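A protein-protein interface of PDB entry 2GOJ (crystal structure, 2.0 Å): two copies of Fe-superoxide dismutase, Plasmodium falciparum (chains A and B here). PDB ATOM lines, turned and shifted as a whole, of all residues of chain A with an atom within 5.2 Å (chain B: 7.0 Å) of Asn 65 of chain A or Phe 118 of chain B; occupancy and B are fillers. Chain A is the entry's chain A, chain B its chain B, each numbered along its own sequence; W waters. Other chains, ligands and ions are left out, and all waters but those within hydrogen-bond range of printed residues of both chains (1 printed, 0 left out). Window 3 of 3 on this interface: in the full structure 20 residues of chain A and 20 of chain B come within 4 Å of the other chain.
Water W1 lies within hydrogen-bond range of OD1 of Asp 140 of chain B (2.6 Å), OD1 of Asp 140 of chain A (2.6 Å), N of Ser 120 of chain B (3.0 Å) and NE2 of His 139 of chain B (3.4 Å).
A ring nitrogen (NE2) of His 139 of chain B lies within hydrogen-bond range of the side-chain carboxylate (OD1) of Asp 140 of chain A (3.0 Å).
NE2 of His 117 of chain B is in hydrogen-bond range of ND1 of His 139 of chain B, 3.0 Å away. The backbone carbonyl oxygen of Asp 140 of chain A is in hydrogen-bond range of the indole nitrogen of Trp 159 of chain A, at 3.1 Å. O of Ser 120 of chain B sits at hydrogen-bond distance from ND1 of His 139 of chain B, 3.0 Å away. The side-chain hydroxyl (OH) of Tyr 34 of chain A lies within hydrogen-bond range of the side-chain amide nitrogen (NE2) of Gln 69 of chain A, 3.2 Å away.
1 position is printed for both chains.
Printed residues of chain A that touch a printed residue of chain B: Tyr 34, Asn 65, Gln 69, Asp 140, Ala 141 and Trp 159. Hydrophobic or aromatic side chains of chain A that line the printed part of chain B: Tyr 34, Ala 141 and Trp 159. Of the 14 printed residues of chain B, 3 touch a printed residue of chain A. Among the printed residues, no Asp or Glu carboxylate lies within 4 Å of a Lys or Arg side-chain nitrogen of the other chain.
Among the printed residues, merely in contact across the chains: Tyr 34 of chain A with Phe 118 of chain B (3.9 Å), Asn 65 of chain A with Phe 118 of chain B (3.4 Å), Gln 69 of chain A with Phe 118 of chain B (3.5 Å), Asp 140 of chain A with Phe 118 of chain B (3.8 Å), Asp 140 of chain A with Gly 119 of chain B (3.8 Å), Ala 141 of chain A with Phe 118 of chain B (3.7 Å), Trp 159 of chain A with Phe 118 of chain B (3.6 Å) and Trp 159 of chain A with Gly 119 of chain B (3.6 Å).
Phe 118 of chain B touches just these residues of chain A: Tyr 34 (3.9 Å), Asn 65 (3.4 Å), Gln 69 (3.5 Å), Asp 140 (3.8 Å), Ala 141 (3.7 Å) and Trp 159 (3.6 Å). Printed residues of chain B within 4 Å of Ala 141 of chain A: Phe 118. Of the printed residues of chain B, Tyr 34 of chain A touches Phe 118. Of the printed residues of chain A, His 139 of chain B touches Asp 140. The nearest printed residue of chain A that does not touch Phe 118 of chain B is Asn 66 of chain A (5.4 Å).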
ATOM      1  N   TYR A  34      18.050 -13.313 -28.523  1.00  0.00           N
ATOM      2  CA  TYR A  34      18.179 -11.898 -28.209  1.00  0.00           C
ATOM      3  C   TYR A  34      19.584 -11.404 -28.549  1.00  0.00           C
ATOM      4  O   TYR A  34      19.733 -10.297 -29.042  1.00  0.00           O
ATOM      5  CB  TYR A  34      17.869 -11.609 -26.734  1.00  0.00           C
ATOM      6  CG  TYR A  34      16.421 -11.845 -26.343  1.00  0.00           C
ATOM      7  CD1 TYR A  34      15.398 -11.102 -26.922  1.00  0.00           C
ATOM      8  CD2 TYR A  34      16.082 -12.804 -25.391  1.00  0.00           C
ATOM      9  CE1 TYR A  34      14.077 -11.308 -26.571  1.00  0.00           C
ATOM     10  CE2 TYR A  34      14.750 -13.018 -25.021  1.00  0.00           C
ATOM     11  CZ  TYR A  34      13.759 -12.271 -25.617  1.00  0.00           C
ATOM     12  OH  TYR A  34      12.452 -12.466 -25.264  1.00  0.00           O
ATOM     13  N   GLY A  61      13.305   1.371 -27.914  1.00  0.00           N
ATOM     14  CA  GLY A  61      12.779   0.562 -29.004  1.00  0.00           C
ATOM     15  C   GLY A  61      13.313  -0.863 -28.996  1.00  0.00           C
ATOM     16  O   GLY A  61      13.536  -1.441 -27.922  1.00  0.00           O
ATOM     17  N   ALA A  62      13.515  -1.429 -30.187  1.00  0.00           N
ATOM     18  CA  ALA A  62      13.948  -2.820 -30.336  1.00  0.00           C
ATOM     19  C   ALA A  62      15.352  -3.074 -29.772  1.00  0.00           C
ATOM     20  O   ALA A  62      15.638  -4.170 -29.309  1.00  0.00           O
ATOM     21  CB  ALA A  62      13.896  -3.244 -31.811  1.00  0.00           C
ATOM     22  N   ILE A  63      16.223  -2.072 -29.836  1.00  0.00           N
ATOM     23  CA  ILE A  63      17.582  -2.216 -29.314  1.00  0.00           C
ATOM     24  C   ILE A  63      17.528  -2.407 -27.801  1.00  0.00           C
ATOM     25  O   ILE A  63      18.191  -3.277 -27.272  1.00  0.00           O
ATOM     26  CB  ILE A  63      18.488  -0.998 -29.690  1.00  0.00           C
ATOM     27  CG1 ILE A  63      18.814  -1.023 -31.190  1.00  0.00           C
ATOM     28  CG2 ILE A  63      19.796  -1.021 -28.874  1.00  0.00           C
ATOM     29  CD1 ILE A  63      19.559   0.249 -31.688  1.00  0.00           C
ATOM     30  N   PHE A  64      16.731  -1.595 -27.119  1.00  0.00           N
ATOM     31  CA  PHE A  64      16.552  -1.745 -25.684  1.00  0.00           C
ATOM     32  C   PHE A  64      15.950  -3.111 -25.362  1.00  0.00           C
ATOM     33  O   PHE A  64      16.441  -3.810 -24.492  1.00  0.00           O
ATOM     34  CB  PHE A  64      15.679  -0.631 -25.096  1.00  0.00           C
ATOM     35  CG  PHE A  64      15.327  -0.857 -23.642  1.00  0.00           C
ATOM     36  CD1 PHE A  64      16.202  -0.474 -22.639  1.00  0.00           C
ATOM     37  CD2 PHE A  64      14.152  -1.510 -23.290  1.00  0.00           C
ATOM     38  CE1 PHE A  64      15.903  -0.709 -21.311  1.00  0.00           C
ATOM     39  CE2 PHE A  64      13.840  -1.754 -21.966  1.00  0.00           C
ATOM     40  CZ  PHE A  64      14.709  -1.361 -20.971  1.00  0.00           C
ATOM     41  N   ASN A  65      14.882  -3.484 -26.065  1.00  0.00           N
ATOM     42  CA  ASN A  65      14.183  -4.729 -25.775  1.00  0.00           C
ATOM     43  C   ASN A  65      15.140  -5.925 -25.787  1.00  0.00           C
ATOM     44  O   ASN A  65      15.159  -6.723 -24.856  1.00  0.00           O
ATOM     45  CB  ASN A  65      13.027  -4.952 -26.771  1.00  0.00           C
ATOM     46  CG  ASN A  65      11.808  -4.042 -26.499  1.00  0.00           C
ATOM     47  OD1 ASN A  65      11.677  -3.433 -25.426  1.00  0.00           O
ATOM     48  ND2 ASN A  65      10.912  -3.964 -27.477  1.00  0.00           N
ATOM     49  N   ASN A  66      15.933  -6.044 -26.848  1.00  0.00           N
ATOM     50  CA  ASN A  66      16.856  -7.148 -26.984  1.00  0.00           C
ATOM     51  C   ASN A  66      18.022  -7.050 -25.994  1.00  0.00           C
ATOM     52  O   ASN A  66      18.407  -8.046 -25.395  1.00  0.00           O
ATOM     53  CB  ASN A  66      17.364  -7.240 -28.425  1.00  0.00           C
ATOM     54  CG  ASN A  66      16.290  -7.712 -29.383  1.00  0.00           C
ATOM     55  OD1 ASN A  66      15.965  -8.892 -29.418  1.00  0.00           O
ATOM     56  ND2 ASN A  66      15.727  -6.792 -30.158  1.00  0.00           N
ATOM     57  N   ALA A  67      18.555  -5.847 -25.803  1.00  0.00           N
ATOM     58  CA  ALA A  67      19.668  -5.633 -24.883  1.00  0.00           C
ATOM     59  C   ALA A  67      19.265  -5.945 -23.446  1.00  0.00           C
ATOM     60  O   ALA A  67      19.956  -6.682 -22.754  1.00  0.00           O
ATOM     61  CB  ALA A  67      20.169  -4.207 -24.984  1.00  0.00           C
ATOM     62  N   ALA A  68      18.142  -5.386 -23.003  1.00  0.00           N
ATOM     63  CA  ALA A  68      17.662  -5.610 -21.639  1.00  0.00           C
ATOM     64  C   ALA A  68      17.316  -7.067 -21.398  1.00  0.00           C
ATOM     65  O   ALA A  68      17.590  -7.586 -20.329  1.00  0.00           O
ATOM     66  CB  ALA A  68      16.489  -4.729 -21.332  1.00  0.00           C
ATOM     67  N   GLN A  69      16.742  -7.734 -22.399  1.00  0.00           N
ATOM     68  CA  GLN A  69      16.437  -9.159 -22.284  1.00  0.00           C
ATOM     69  C   GLN A  69      17.699 -10.005 -22.127  1.00  0.00           C
ATOM     70  O   GLN A  69      17.689 -10.990 -21.395  1.00  0.00           O
ATOM     71  CB  GLN A  69      15.598  -9.677 -23.468  1.00  0.00           C
ATOM     72  CG  GLN A  69      14.117  -9.288 -23.409  1.00  0.00           C
ATOM     73  CD  GLN A  69      13.382  -9.888 -22.220  1.00  0.00           C
ATOM     74  OE1 GLN A  69      13.478  -9.379 -21.104  1.00  0.00           O
ATOM     75  NE2 GLN A  69      12.629 -10.952 -22.462  1.00  0.00           N
ATOM     76  N   ILE A  70      18.766  -9.642 -22.822  1.00  0.00           N
ATOM     77  CA  ILE A  70      20.026 -10.365 -22.699  1.00  0.00           C
ATOM     78  C   ILE A  70      20.503 -10.190 -21.264  1.00  0.00           C
ATOM     79  O   ILE A  70      20.824 -11.165 -20.602  1.00  0.00           O
ATOM     80  CB  ILE A  70      21.110  -9.832 -23.669  1.00  0.00           C
ATOM     81  CG1 ILE A  70      20.729 -10.066 -25.133  1.00  0.00           C
ATOM     82  CG2 ILE A  70      22.426 -10.539 -23.409  1.00  0.00           C
ATOM     83  CD1 ILE A  70      21.518  -9.171 -26.106  1.00  0.00           C
ATOM     84  N   ASP A 140       7.587  -6.774 -19.647  1.00  0.00           N
ATOM     85  CA  ASP A 140       8.328  -7.057 -20.868  1.00  0.00           C
ATOM     86  C   ASP A 140       9.842  -7.105 -20.608  1.00  0.00           C
ATOM     87  O   ASP A 140      10.302  -7.975 -19.861  1.00  0.00           O
ATOM     88  CB  ASP A 140       7.925  -6.060 -21.974  1.00  0.00           C
ATOM     89  CG  ASP A 140       6.447  -6.128 -22.301  1.00  0.00           C
ATOM     90  OD1 ASP A 140       5.859  -7.226 -22.287  1.00  0.00           O
ATOM     91  OD2 ASP A 140       5.784  -5.126 -22.583  1.00  0.00           O
ATOM     92  N   ALA A 141      10.617  -6.189 -21.180  1.00  0.00           N
ATOM     93  CA  ALA A 141      12.086  -6.192 -20.990  1.00  0.00           C
ATOM     94  C   ALA A 141      12.547  -5.204 -19.920  1.00  0.00           C
ATOM     95  O   ALA A 141      13.751  -5.011 -19.717  1.00  0.00           O
ATOM     96  CB  ALA A 141      12.782  -5.895 -22.301  1.00  0.00           C
ATOM     97  N   TRP A 159       7.718 -14.338 -17.873  1.00  0.00           N
ATOM     98  CA  TRP A 159       7.276 -14.589 -19.243  1.00  0.00           C
ATOM     99  C   TRP A 159       6.823 -16.044 -19.275  1.00  0.00           C
ATOM    100  O   TRP A 159       7.423 -16.891 -18.624  1.00  0.00           O
ATOM    101  CB  TRP A 159       8.425 -14.421 -20.237  1.00  0.00           C
ATOM    102  CG  TRP A 159       8.812 -13.008 -20.576  1.00  0.00           C
ATOM    103  CD1 TRP A 159       9.311 -12.054 -19.724  1.00  0.00           C
ATOM    104  CD2 TRP A 159       8.781 -12.411 -21.871  1.00  0.00           C
ATOM    105  NE1 TRP A 159       9.577 -10.902 -20.418  1.00  0.00           N
ATOM    106  CE2 TRP A 159       9.253 -11.093 -21.738  1.00  0.00           C
ATOM    107  CE3 TRP A 159       8.382 -12.860 -23.142  1.00  0.00           C
ATOM    108  CZ2 TRP A 159       9.345 -10.214 -22.823  1.00  0.00           C
ATOM    109  CZ3 TRP A 159       8.467 -11.987 -24.222  1.00  0.00           C
ATOM    110  CH2 TRP A 159       8.955 -10.677 -24.053  1.00  0.00           C
ATOM    111  N   ILE B 113       4.119  -8.357 -38.719  1.00  0.00           N
ATOM    112  CA  ILE B 113       3.696  -7.657 -37.509  1.00  0.00           C
ATOM    113  C   ILE B 113       3.420  -8.621 -36.350  1.00  0.00           C
ATOM    114  O   ILE B 113       3.809  -8.341 -35.212  1.00  0.00           O
ATOM    115  CB  ILE B 113       2.494  -6.729 -37.822  1.00  0.00           C
ATOM    116  CG1 ILE B 113       3.007  -5.480 -38.565  1.00  0.00           C
ATOM    117  CG2 ILE B 113       1.757  -6.320 -36.558  1.00  0.00           C
ATOM    118  CD1 ILE B 113       2.087  -4.973 -39.621  1.00  0.00           C
ATOM    119  N   LEU B 114       2.781  -9.751 -36.643  1.00  0.00           N
ATOM    120  CA  LEU B 114       2.534 -10.793 -35.650  1.00  0.00           C
ATOM    121  C   LEU B 114       3.850 -11.362 -35.120  1.00  0.00           C
ATOM    122  O   LEU B 114       3.995 -11.557 -33.921  1.00  0.00           O
ATOM    123  CB  LEU B 114       1.698 -11.925 -36.237  1.00  0.00           C
ATOM    124  CG  LEU B 114       0.223 -11.623 -36.536  1.00  0.00           C
ATOM    125  CD1 LEU B 114      -0.367 -12.789 -37.317  1.00  0.00           C
ATOM    126  CD2 LEU B 114      -0.554 -11.402 -35.264  1.00  0.00           C
ATOM    127  N   CYS B 115       4.802 -11.611 -36.016  1.00  0.00           N
ATOM    128  CA  CYS B 115       6.107 -12.140 -35.633  1.00  0.00           C
ATOM    129  C   CYS B 115       6.983 -11.079 -34.950  1.00  0.00           C
ATOM    130  O   CYS B 115       7.791 -11.412 -34.094  1.00  0.00           O
ATOM    131  CB  CYS B 115       6.834 -12.736 -36.843  1.00  0.00           C
ATOM    132  SG  CYS B 115       6.122 -14.288 -37.492  1.00  0.00           S
ATOM    133  N   GLY B 116       6.816  -9.809 -35.319  1.00  0.00           N
ATOM    134  CA  GLY B 116       7.646  -8.735 -34.793  1.00  0.00           C
ATOM    135  C   GLY B 116       7.227  -8.240 -33.411  1.00  0.00           C
ATOM    136  O   GLY B 116       7.987  -7.527 -32.749  1.00  0.00           O
ATOM    137  N   HIS B 117       6.034  -8.617 -32.955  1.00  0.00           N
ATOM    138  CA  HIS B 117       5.496  -8.030 -31.741  1.00  0.00           C
ATOM    139  C   HIS B 117       6.266  -8.484 -30.473  1.00  0.00           C
ATOM    140  O   HIS B 117       6.411  -9.677 -30.225  1.00  0.00           O
ATOM    141  CB  HIS B 117       3.989  -8.324 -31.593  1.00  0.00           C
ATOM    142  CG  HIS B 117       3.402  -7.678 -30.389  1.00  0.00           C
ATOM    143  ND1 HIS B 117       3.190  -6.322 -30.321  1.00  0.00           N
ATOM    144  CD2 HIS B 117       3.099  -8.170 -29.163  1.00  0.00           C
ATOM    145  CE1 HIS B 117       2.739  -6.011 -29.116  1.00  0.00           C
ATOM    146  NE2 HIS B 117       2.674  -7.116 -28.395  1.00  0.00           N
ATOM    147  N   PHE B 118       6.755  -7.537 -29.681  1.00  0.00           N
ATOM    148  CA  PHE B 118       7.533  -7.875 -28.488  1.00  0.00           C
ATOM    149  C   PHE B 118       6.642  -7.979 -27.260  1.00  0.00           C
ATOM    150  O   PHE B 118       5.923  -7.061 -26.943  1.00  0.00           O
ATOM    151  CB  PHE B 118       8.659  -6.861 -28.231  1.00  0.00           C
ATOM    152  CG  PHE B 118       9.561  -7.246 -27.087  1.00  0.00           C
ATOM    153  CD1 PHE B 118      10.461  -8.295 -27.219  1.00  0.00           C
ATOM    154  CD2 PHE B 118       9.502  -6.569 -25.877  1.00  0.00           C
ATOM    155  CE1 PHE B 118      11.291  -8.664 -26.161  1.00  0.00           C
ATOM    156  CE2 PHE B 118      10.336  -6.939 -24.816  1.00  0.00           C
ATOM    157  CZ  PHE B 118      11.220  -7.990 -24.965  1.00  0.00           C
ATOM    158  N   GLY B 119       6.720  -9.105 -26.566  1.00  0.00           N
ATOM    159  CA  GLY B 119       5.892  -9.371 -25.419  1.00  0.00           C
ATOM    160  C   GLY B 119       4.554  -9.973 -25.802  1.00  0.00           C
ATOM    161  O   GLY B 119       4.367 -10.466 -26.927  1.00  0.00           O
ATOM    162  N   SER B 120       3.627  -9.934 -24.847  1.00  0.00           N
ATOM    163  CA  SER B 120       2.298 -10.499 -25.010  1.00  0.00           C
ATOM    164  C   SER B 120       1.429  -9.539 -25.803  1.00  0.00           C
ATOM    165  O   SER B 120       1.565  -8.316 -25.678  1.00  0.00           O
ATOM    166  CB  SER B 120       1.658 -10.763 -23.640  1.00  0.00           C
ATOM    167  OG  SER B 120       2.445 -11.642 -22.828  1.00  0.00           O
ATOM    168  N   GLY B 121       0.515 -10.073 -26.609  1.00  0.00           N
ATOM    169  CA  GLY B 121      -0.333  -9.207 -27.403  1.00  0.00           C
ATOM    170  C   GLY B 121      -1.178  -9.867 -28.461  1.00  0.00           C
ATOM    171  O   GLY B 121      -1.353 -11.089 -28.489  1.00  0.00           O
ATOM    172  N   GLN B 137      -1.623  -3.740 -34.001  1.00  0.00           N
ATOM    173  CA  GLN B 137      -1.124  -4.592 -32.940  1.00  0.00           C
ATOM    174  C   GLN B 137      -1.390  -3.926 -31.588  1.00  0.00           C
ATOM    175  O   GLN B 137      -1.295  -2.698 -31.441  1.00  0.00           O
ATOM    176  CB  GLN B 137       0.366  -4.902 -33.141  1.00  0.00           C
ATOM    177  CG  GLN B 137       1.272  -3.713 -32.973  1.00  0.00           C
ATOM    178  CD  GLN B 137       2.651  -3.951 -33.523  1.00  0.00           C
ATOM    179  OE1 GLN B 137       3.331  -4.908 -33.135  1.00  0.00           O
ATOM    180  NE2 GLN B 137       3.081  -3.085 -34.421  1.00  0.00           N
ATOM    181  N   HIS B 139      -0.907  -4.546 -27.141  1.00  0.00           N
ATOM    182  CA  HIS B 139      -0.097  -5.192 -26.130  1.00  0.00           C
ATOM    183  C   HIS B 139      -0.996  -5.730 -25.033  1.00  0.00           C
ATOM    184  O   HIS B 139      -2.019  -5.125 -24.709  1.00  0.00           O
ATOM    185  CB  HIS B 139       0.904  -4.188 -25.552  1.00  0.00           C
ATOM    186  CG  HIS B 139       2.125  -4.828 -24.986  1.00  0.00           C
ATOM    187  ND1 HIS B 139       2.923  -5.683 -25.718  1.00  0.00           N
ATOM    188  CD2 HIS B 139       2.684  -4.749 -23.758  1.00  0.00           C
ATOM    189  CE1 HIS B 139       3.915  -6.108 -24.960  1.00  0.00           C
ATOM    190  NE2 HIS B 139       3.793  -5.555 -23.769  1.00  0.00           N
ATOM    191  N   ASP B 140      -0.614  -6.865 -24.474  1.00  0.00           N
ATOM    192  CA  ASP B 140      -1.288  -7.450 -23.332  1.00  0.00           C
ATOM    193  C   ASP B 140      -2.780  -7.683 -23.627  1.00  0.00           C
ATOM    194  O   ASP B 140      -3.089  -8.507 -24.470  1.00  0.00           O
ATOM    195  CB  ASP B 140      -1.017  -6.591 -22.094  1.00  0.00           C
ATOM    196  CG  ASP B 140       0.465  -6.547 -21.738  1.00  0.00           C
ATOM    197  OD1 ASP B 140       1.187  -7.509 -22.069  1.00  0.00           O
ATOM    198  OD2 ASP B 140       0.999  -5.600 -21.126  1.00  0.00           O
ATOM    199  N   ILE B 158      -1.013 -13.692 -29.925  1.00  0.00           N
ATOM    200  CA  ILE B 158       0.406 -14.052 -29.953  1.00  0.00           C
ATOM    201  C   ILE B 158       1.047 -14.057 -28.550  1.00  0.00           C
ATOM    202  O   ILE B 158       2.265 -14.112 -28.434  1.00  0.00           O
ATOM    203  CB  ILE B 158       1.245 -13.225 -30.992  1.00  0.00           C
ATOM    204  CG1 ILE B 158       1.025 -11.712 -30.863  1.00  0.00           C
ATOM    205  CG2 ILE B 158       0.962 -13.693 -32.434  1.00  0.00           C
ATOM    206  CD1 ILE B 158       1.827 -11.091 -29.760  1.00  0.00           C
ATOM    207  N   ARG B 171       7.355 -18.799 -33.048  1.00  0.00           N
ATOM    208  CA  ARG B 171       6.110 -18.096 -33.305  1.00  0.00           C
ATOM    209  C   ARG B 171       5.816 -18.020 -34.806  1.00  0.00           C
ATOM    210  O   ARG B 171       4.654 -18.032 -35.216  1.00  0.00           O
ATOM    211  CB  ARG B 171       6.154 -16.687 -32.721  1.00  0.00           C
ATOM    212  CG  ARG B 171       4.828 -15.972 -32.804  1.00  0.00           C
ATOM    213  CD  ARG B 171       4.939 -14.482 -32.581  1.00  0.00           C
ATOM    214  NE  ARG B 171       5.251 -14.174 -31.193  1.00  0.00           N
ATOM    215  CZ  ARG B 171       5.517 -12.951 -30.753  1.00  0.00           C
ATOM    216  NH1 ARG B 171       5.497 -11.922 -31.592  1.00  0.00           N
ATOM    217  NH2 ARG B 171       5.797 -12.754 -29.471  1.00  0.00           N
HETATM  218  O   HOH W   1       3.570  -8.535 -22.203  1.00  0.00           O
